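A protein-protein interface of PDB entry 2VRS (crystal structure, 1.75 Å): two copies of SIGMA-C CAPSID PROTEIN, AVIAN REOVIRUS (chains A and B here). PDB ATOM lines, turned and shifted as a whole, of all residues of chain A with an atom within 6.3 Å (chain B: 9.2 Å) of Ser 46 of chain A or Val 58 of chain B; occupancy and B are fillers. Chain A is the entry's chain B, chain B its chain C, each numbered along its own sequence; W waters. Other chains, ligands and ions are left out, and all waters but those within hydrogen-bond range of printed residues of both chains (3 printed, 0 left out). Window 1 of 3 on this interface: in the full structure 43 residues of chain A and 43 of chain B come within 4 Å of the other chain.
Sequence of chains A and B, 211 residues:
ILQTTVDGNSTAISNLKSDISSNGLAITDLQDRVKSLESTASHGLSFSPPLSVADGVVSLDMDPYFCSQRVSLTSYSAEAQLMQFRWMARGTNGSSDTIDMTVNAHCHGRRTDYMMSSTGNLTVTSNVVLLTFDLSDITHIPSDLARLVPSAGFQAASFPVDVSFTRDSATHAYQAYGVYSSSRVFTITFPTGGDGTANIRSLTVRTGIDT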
ATOM      1  N   GLY A  44      30.779 -22.097  20.442  1.00  0.00           N
ATOM      2  CA  GLY A  44      30.377 -20.690  20.297  1.00  0.00           C
ATOM      3  C   GLY A  44      29.437 -20.081  21.345  1.00  0.00           C
ATOM      4  O   GLY A  44      28.856 -19.010  21.085  1.00  0.00           O
ATOM      5  N   LEU A  45      29.287 -20.714  22.525  1.00  0.00           N
ATOM      6  CA  LEU A  45      28.133 -20.372  23.410  1.00  0.00           C
ATOM      7  C   LEU A  45      28.317 -19.176  24.304  1.00  0.00           C
ATOM      8  O   LEU A  45      29.319 -19.089  25.041  1.00  0.00           O
ATOM      9  CB  LEU A  45      27.708 -21.550  24.295  1.00  0.00           C
ATOM     10  CG  LEU A  45      27.043 -22.753  23.643  1.00  0.00           C
ATOM     11  CD1 LEU A  45      26.751 -23.787  24.691  1.00  0.00           C
ATOM     12  CD2 LEU A  45      25.793 -22.432  22.847  1.00  0.00           C
ATOM     13  N   SER A  46      27.309 -18.284  24.281  1.00  0.00           N
ATOM     14  CA  SER A  46      27.201 -17.182  25.229  1.00  0.00           C
ATOM     15  C   SER A  46      25.765 -17.232  25.804  1.00  0.00           C
ATOM     16  O   SER A  46      24.938 -18.035  25.340  1.00  0.00           O
ATOM     17  CB  SER A  46      27.487 -15.804  24.607  1.00  0.00           C
ATOM     18  OG  SER A  46      26.661 -15.556  23.480  1.00  0.00           O
ATOM     19  N   PHE A  47      25.518 -16.369  26.784  1.00  0.00           N
ATOM     20  CA  PHE A  47      24.271 -16.395  27.568  1.00  0.00           C
ATOM     21  C   PHE A  47      23.717 -14.993  27.717  1.00  0.00           C
ATOM     22  O   PHE A  47      24.463 -14.077  28.077  1.00  0.00           O
ATOM     23  CB  PHE A  47      24.549 -17.068  28.925  1.00  0.00           C
ATOM     24  CG  PHE A  47      24.975 -18.518  28.798  1.00  0.00           C
ATOM     25  CD1 PHE A  47      24.027 -19.542  28.702  1.00  0.00           C
ATOM     26  CD2 PHE A  47      26.351 -18.851  28.689  1.00  0.00           C
ATOM     27  CE1 PHE A  47      24.398 -20.881  28.550  1.00  0.00           C
ATOM     28  CE2 PHE A  47      26.744 -20.208  28.517  1.00  0.00           C
ATOM     29  CZ  PHE A  47      25.762 -21.224  28.444  1.00  0.00           C
ATOM     30  N   SER A  48      22.423 -14.819  27.386  1.00  0.00           N
ATOM     31  CA  SER A  48      21.751 -13.504  27.412  1.00  0.00           C
ATOM     32  C   SER A  48      21.007 -13.347  28.736  1.00  0.00           C
ATOM     33  O   SER A  48      20.422 -14.318  29.197  1.00  0.00           O
ATOM     34  CB  SER A  48      20.714 -13.415  26.299  1.00  0.00           C
ATOM     35  OG  SER A  48      21.328 -13.097  25.078  1.00  0.00           O
ATOM     36  N   PRO A  49      21.020 -12.141  29.337  1.00  0.00           N
ATOM     37  CA  PRO A  49      20.229 -11.902  30.572  1.00  0.00           C
ATOM     38  C   PRO A  49      18.780 -12.388  30.370  1.00  0.00           C
ATOM     39  O   PRO A  49      18.190 -12.150  29.321  1.00  0.00           O
ATOM     40  CB  PRO A  49      20.273 -10.375  30.723  1.00  0.00           C
ATOM     41  CG  PRO A  49      21.582 -10.011  30.105  1.00  0.00           C
ATOM     42  CD  PRO A  49      21.749 -10.930  28.925  1.00  0.00           C
ATOM     43  N   LEU A  51      20.058 -14.985  31.955  1.00  0.00           N
ATOM     44  CA  LEU A  51      21.136 -15.972  32.073  1.00  0.00           C
ATOM     45  C   LEU A  51      22.484 -15.258  32.119  1.00  0.00           C
ATOM     46  O   LEU A  51      22.685 -14.247  31.438  1.00  0.00           O
ATOM     47  CB  LEU A  51      21.078 -16.978  30.920  1.00  0.00           C
ATOM     48  CG  LEU A  51      19.778 -17.735  30.650  1.00  0.00           C
ATOM     49  CD1 LEU A  51      19.888 -18.658  29.375  1.00  0.00           C
ATOM     50  CD2 LEU A  51      19.323 -18.545  31.872  1.00  0.00           C
ATOM     51  N   VAL A  53      26.988 -15.999  33.138  1.00  0.00           N
ATOM     52  CA  VAL A  53      28.025 -16.972  33.467  1.00  0.00           C
ATOM     53  C   VAL A  53      29.148 -16.273  34.260  1.00  0.00           C
ATOM     54  O   VAL A  53      29.494 -15.120  33.990  1.00  0.00           O
ATOM     55  CB  VAL A  53      28.527 -17.717  32.207  1.00  0.00           C
ATOM     56  CG1 VAL A  53      29.061 -16.745  31.163  1.00  0.00           C
ATOM     57  CG2 VAL A  53      29.567 -18.783  32.591  1.00  0.00           C
ATOM     58  N   LEU B  45      26.002 -30.330  24.040  1.00  0.00           N
ATOM     59  CA  LEU B  45      24.914 -29.699  24.825  1.00  0.00           C
ATOM     60  C   LEU B  45      23.776 -29.170  23.957  1.00  0.00           C
ATOM     61  O   LEU B  45      24.004 -28.572  22.885  1.00  0.00           O
ATOM     62  CB  LEU B  45      25.453 -28.543  25.669  1.00  0.00           C
ATOM     63  CG  LEU B  45      26.331 -28.712  26.903  1.00  0.00           C
ATOM     64  CD1 LEU B  45      26.782 -27.337  27.347  1.00  0.00           C
ATOM     65  CD2 LEU B  45      25.677 -29.430  28.057  1.00  0.00           C
ATOM     66  N   SER B  46      22.539 -29.348  24.448  1.00  0.00           N
ATOM     67  CA  SER B  46      21.376 -28.773  23.816  1.00  0.00           C
ATOM     68  C   SER B  46      20.558 -28.134  24.936  1.00  0.00           C
ATOM     69  O   SER B  46      20.820 -28.371  26.113  1.00  0.00           O
ATOM     70  CB  SER B  46      20.523 -29.844  23.100  1.00  0.00           C
ATOM     71  OG  SER B  46      20.162 -30.939  23.942  1.00  0.00           O
ATOM     72  N   PHE B  47      19.548 -27.404  24.531  1.00  0.00           N
ATOM     73  CA  PHE B  47      18.767 -26.613  25.476  1.00  0.00           C
ATOM     74  C   PHE B  47      17.285 -26.860  25.240  1.00  0.00           C
ATOM     75  O   PHE B  47      16.804 -26.811  24.100  1.00  0.00           O
ATOM     76  CB  PHE B  47      19.183 -25.138  25.341  1.00  0.00           C
ATOM     77  CG  PHE B  47      20.620 -24.894  25.733  1.00  0.00           C
ATOM     78  CD1 PHE B  47      21.660 -25.098  24.804  1.00  0.00           C
ATOM     79  CD2 PHE B  47      20.947 -24.505  27.021  1.00  0.00           C
ATOM     80  CE1 PHE B  47      22.996 -24.907  25.163  1.00  0.00           C
ATOM     81  CE2 PHE B  47      22.277 -24.312  27.395  1.00  0.00           C
ATOM     82  CZ  PHE B  47      23.319 -24.537  26.451  1.00  0.00           C
ATOM     83  N   SER B  48      16.558 -27.154  26.324  1.00  0.00           N
ATOM     84  CA  SER B  48      15.121 -27.423  26.229  1.00  0.00           C
ATOM     85  C   SER B  48      14.302 -26.188  26.607  1.00  0.00           C
ATOM     86  O   SER B  48      14.711 -25.423  27.475  1.00  0.00           O
ATOM     87  CB  SER B  48      14.720 -28.579  27.146  1.00  0.00           C
ATOM     88  OG  SER B  48      15.075 -28.242  28.468  1.00  0.00           O
ATOM     89  N   PRO B  50      11.891 -23.675  28.391  1.00  0.00           N
ATOM     90  CA  PRO B  50      11.942 -22.392  27.694  1.00  0.00           C
ATOM     91  C   PRO B  50      13.326 -21.817  27.407  1.00  0.00           C
ATOM     92  O   PRO B  50      13.430 -20.623  27.091  1.00  0.00           O
ATOM     93  CB  PRO B  50      11.206 -21.444  28.663  1.00  0.00           C
ATOM     94  CG  PRO B  50      11.588 -22.023  30.034  1.00  0.00           C
ATOM     95  CD  PRO B  50      11.731 -23.518  29.850  1.00  0.00           C
ATOM     96  N   LEU B  51      14.385 -22.625  27.524  1.00  0.00           N
ATOM     97  CA  LEU B  51      15.711 -22.166  27.064  1.00  0.00           C
ATOM     98  C   LEU B  51      15.843 -22.390  25.554  1.00  0.00           C
ATOM     99  O   LEU B  51      15.253 -23.316  24.998  1.00  0.00           O
ATOM    100  CB  LEU B  51      16.829 -22.917  27.789  1.00  0.00           C
ATOM    101  CG  LEU B  51      16.825 -22.939  29.314  1.00  0.00           C
ATOM    102  CD1 LEU B  51      17.876 -23.902  29.834  1.00  0.00           C
ATOM    103  CD2 LEU B  51      17.056 -21.582  29.864  1.00  0.00           C
ATOM    104  N   SER B  52      16.579 -21.514  24.882  1.00  0.00           N
ATOM    105  CA  SER B  52      16.754 -21.693  23.433  1.00  0.00           C
ATOM    106  C   SER B  52      18.053 -21.073  22.966  1.00  0.00           C
ATOM    107  O   SER B  52      18.584 -20.191  23.631  1.00  0.00           O
ATOM    108  CB  SER B  52      15.572 -21.127  22.644  1.00  0.00           C
ATOM    109  OG  SER B  52      15.530 -19.703  22.705  1.00  0.00           O
ATOM    110  N   VAL B  53      18.559 -21.552  21.825  1.00  0.00           N
ATOM    111  CA  VAL B  53      19.819 -21.043  21.260  1.00  0.00           C
ATOM    112  C   VAL B  53      19.584 -20.542  19.834  1.00  0.00           C
ATOM    113  O   VAL B  53      18.866 -21.158  19.059  1.00  0.00           O
ATOM    114  CB  VAL B  53      20.917 -22.128  21.216  1.00  0.00           C
ATOM    115  CG1 VAL B  53      22.310 -21.472  21.128  1.00  0.00           C
ATOM    116  CG2 VAL B  53      20.823 -23.013  22.421  1.00  0.00           C
ATOM    117  N   ALA B  54      20.176 -19.399  19.505  1.00  0.00           N
ATOM    118  CA  ALA B  54      20.110 -18.845  18.156  1.00  0.00           C
ATOM    119  C   ALA B  54      21.488 -18.276  17.888  1.00  0.00           C
ATOM    120  O   ALA B  54      21.927 -17.326  18.572  1.00  0.00           O
ATOM    121  CB  ALA B  54      19.052 -17.749  18.070  1.00  0.00           C
ATOM    122  N   ASP B  55      22.195 -18.879  16.930  1.00  0.00           N
ATOM    123  CA  ASP B  55      23.518 -18.383  16.551  1.00  0.00           C
ATOM    124  C   ASP B  55      24.463 -18.382  17.770  1.00  0.00           C
ATOM    125  O   ASP B  55      25.196 -17.418  18.025  1.00  0.00           O
ATOM    126  CB  ASP B  55      23.365 -16.979  15.933  1.00  0.00           C
ATOM    127  CG  ASP B  55      24.647 -16.459  15.296  1.00  0.00           C
ATOM    128  OD1 ASP B  55      25.480 -17.279  14.828  1.00  0.00           O
ATOM    129  OD2 ASP B  55      24.815 -15.219  15.271  1.00  0.00           O
ATOM    130  N   GLY B  56      24.423 -19.477  18.535  1.00  0.00           N
ATOM    131  CA  GLY B  56      25.300 -19.644  19.696  1.00  0.00           C
ATOM    132  C   GLY B  56      24.945 -18.816  20.935  1.00  0.00           C
ATOM    133  O   GLY B  56      25.663 -18.872  21.925  1.00  0.00           O
ATOM    134  N   VAL B  57      23.873 -18.020  20.871  1.00  0.00           N
ATOM    135  CA  VAL B  57      23.433 -17.218  22.019  1.00  0.00           C
ATOM    136  C   VAL B  57      22.276 -17.957  22.712  1.00  0.00           C
ATOM    137  O   VAL B  57      21.245 -18.225  22.089  1.00  0.00           O
ATOM    138  CB  VAL B  57      22.990 -15.788  21.612  1.00  0.00           C
ATOM    139  CG1 VAL B  57      22.579 -14.962  22.847  1.00  0.00           C
ATOM    140  CG2 VAL B  57      24.104 -15.069  20.846  1.00  0.00           C
ATOM    141  N   VAL B  58      22.465 -18.275  23.997  1.00  0.00           N
ATOM    142  CA  VAL B  58      21.440 -18.983  24.756  1.00  0.00           C
ATOM    143  C   VAL B  58      20.607 -17.924  25.492  1.00  0.00           C
ATOM    144  O   VAL B  58      21.159 -16.975  26.109  1.00  0.00           O
ATOM    145  CB  VAL B  58      22.028 -20.008  25.742  1.00  0.00           C
ATOM    146  CG1 VAL B  58      20.911 -20.862  26.407  1.00  0.00           C
ATOM    147  CG2 VAL B  58      23.021 -20.942  25.000  1.00  0.00           C
ATOM    148  N   SER B  59      19.296 -18.085  25.352  1.00  0.00           N
ATOM    149  CA  SER B  59      18.306 -17.148  25.900  1.00  0.00           C
ATOM    150  C   SER B  59      17.283 -17.883  26.738  1.00  0.00           C
ATOM    151  O   SER B  59      17.101 -19.103  26.606  1.00  0.00           O
ATOM    152  CB  SER B  59      17.606 -16.402  24.754  1.00  0.00           C
ATOM    153  OG  SER B  59      18.495 -15.469  24.183  1.00  0.00           O
ATOM    154  N   LEU B  60      16.637 -17.144  27.649  1.00  0.00           N
ATOM    155  CA  LEU B  60      15.399 -17.626  28.261  1.00  0.00           C
ATOM    156  C   LEU B  60      14.249 -16.931  27.539  1.00  0.00           C
ATOM    157  O   LEU B  60      14.184 -15.699  27.546  1.00  0.00           O
ATOM    158  CB  LEU B  60      15.367 -17.279  29.770  1.00  0.00           C
ATOM    159  CG  LEU B  60      14.034 -17.561  30.472  1.00  0.00           C
ATOM    160  CD1 LEU B  60      13.823 -19.115  30.587  1.00  0.00           C
ATOM    161  CD2 LEU B  60      14.085 -16.943  31.854  1.00  0.00           C
ATOM    162  N   ASP B  61      13.370 -17.717  26.898  1.00  0.00           N
ATOM    163  CA  ASP B  61      12.186 -17.188  26.230  1.00  0.00           C
ATOM    164  C   ASP B  61      11.171 -16.897  27.337  1.00  0.00           C
ATOM    165  O   ASP B  61      10.886 -17.785  28.163  1.00  0.00           O
ATOM    166  CB  ASP B  61      11.628 -18.168  25.216  1.00  0.00           C
ATOM    167  CG  ASP B  61      12.589 -18.370  24.036  1.00  0.00           C
ATOM    168  OD1 ASP B  61      13.026 -17.357  23.480  1.00  0.00           O
ATOM    169  OD2 ASP B  61      12.866 -19.524  23.700  1.00  0.00           O
HETATM  170  O   HOH W   1      27.774 -16.592  21.267  1.00  0.00           O
HETATM  171  O   HOH W   2      18.266 -12.837  24.368  1.00  0.00           O
HETATM  172  O   HOH W   3      17.697 -14.458  27.752  1.00  0.00           O
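O of Gly 56 of chain B is in hydrogen-bond range of N of Ser 46 of chain A (2.9 Å). N of Val 58 of chain B is in hydrogen-bond range of O of Ser 46 of chain A, at 2.8 Å. N of Ser 48 of chain A sits at hydrogen-bond distance from O of Val 58 of chain B, 2.8 Å away. O of Gly 44 of chain A lies close to O of Gly 56 of chain B (3.3 Å).
Leu 45 of chain A touches Phe 47 of chain B (CD1 to CZ, 3.9 Å). O of Gly 56 of chain B touches CA of Leu 45 of chain A, 3.2 Å away. Leu 45 of chain A touches Val 58 of chain B. Ser 46 of chain A touches Val 57 of chain B. Phe 47 of chain A touches Val 58 of chain B. Val 57 of chain B touches Ser 48 of chain A (CG1 to OG, 3.2 Å). Ser 59 of chain B touches Ser 48 of chain A (OG to CB, 3.7 Å). Val 58 of chain B touches Leu 51 of chain A. CD1 of Leu 51 of chain A touches C of Ser 59 of chain B (3.8 Å). Leu 60 of chain B touches Leu 51 of chain A.
Printed residues of chain B within 4 Å of Gly 44 of chain A: Gly 56. Of chain B, only Gly 56 (2.9 Å), Val 57 (3.7 Å) and Val 58 (2.8 Å) come within 4 Å of Ser 46 of chain A. Phe 47 of chain A touches just one residue of chain B: Val 58. Of the printed residues of chain B, Leu 51 of chain A touches Val 58, Ser 59 and Leu 60. Of the printed residues of chain A, Gly 56 of chain B touches Gly 44, Leu 45 and Ser 46. Of the printed residues of chain A, Val 57 of chain B touches Ser 46 (3.7 Å) and Ser 48 (3.2 Å). Val 58 of chain B touches just these residues of chain A: Leu 45 (3.8 Å), Ser 46 (2.8 Å), Phe 47 (3.5 Å), Ser 48 (2.8 Å) and Leu 51 (3.8 Å). Of the printed residues of chain A, Leu 60 of chain B touches Leu 51. The nearest residue of chain A that does not touch Val 58 of chain B is Pro 49 of chain A (5.8 Å). The nearest printed residue of chain A that does not touch Leu 60 of chain B is Ser 48 of chain A (5.0 Å).
Hydrophobic or aromatic side chains of chain A within 4 Å of the printed part of chain B: Leu 45, Phe 47 and Leu 51. Of the 16 printed residues of chain B, 6 touch a printed residue of chain A. Printed residues of chain B that touch a printed residue of chain A: Phe 47, Gly 56, Val 57, Val 58, Ser 59 and Leu 60. Among the printed residues, no Asp or Glu carboxylate lies within 4 Å of a Lys or Arg side-chain nitrogen of the other chain.
Leu 45 of chain A touches Phe 47 of chain B, but with the chains exchanged Phe 47 of chain A does not touch Leu 45 of chain B (6.3 Å). 6 positions are printed for both chains. Of the 14 pairs that touch across the chains among the printed residues, none has its exchanged pair printed and touching as well.
Water W2 lies within hydrogen-bond range of OG of Ser 59 of chain B (2.6 Å) and OG of Ser 48 of chain A (3.2 Å). Water W1 lies within hydrogen-bond range of the backbone carbonyl oxygen of Gly 44 of chain A, the side-chain hydroxyl of Ser 46 of chain A and the backbone carbonyl oxygen of Gly 56 of chain B. Water W3 lies within hydrogen-bond range of O of Pro 49 of chain A (2.8 Å), N of Leu 60 of chain B (2.9 Å) and O of Ser 48 of chain A (3.1 Å).
O of Ser 52 of chain B is in hydrogen-bond range of N of Ser 59 of chain B, at 2.8 Å.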
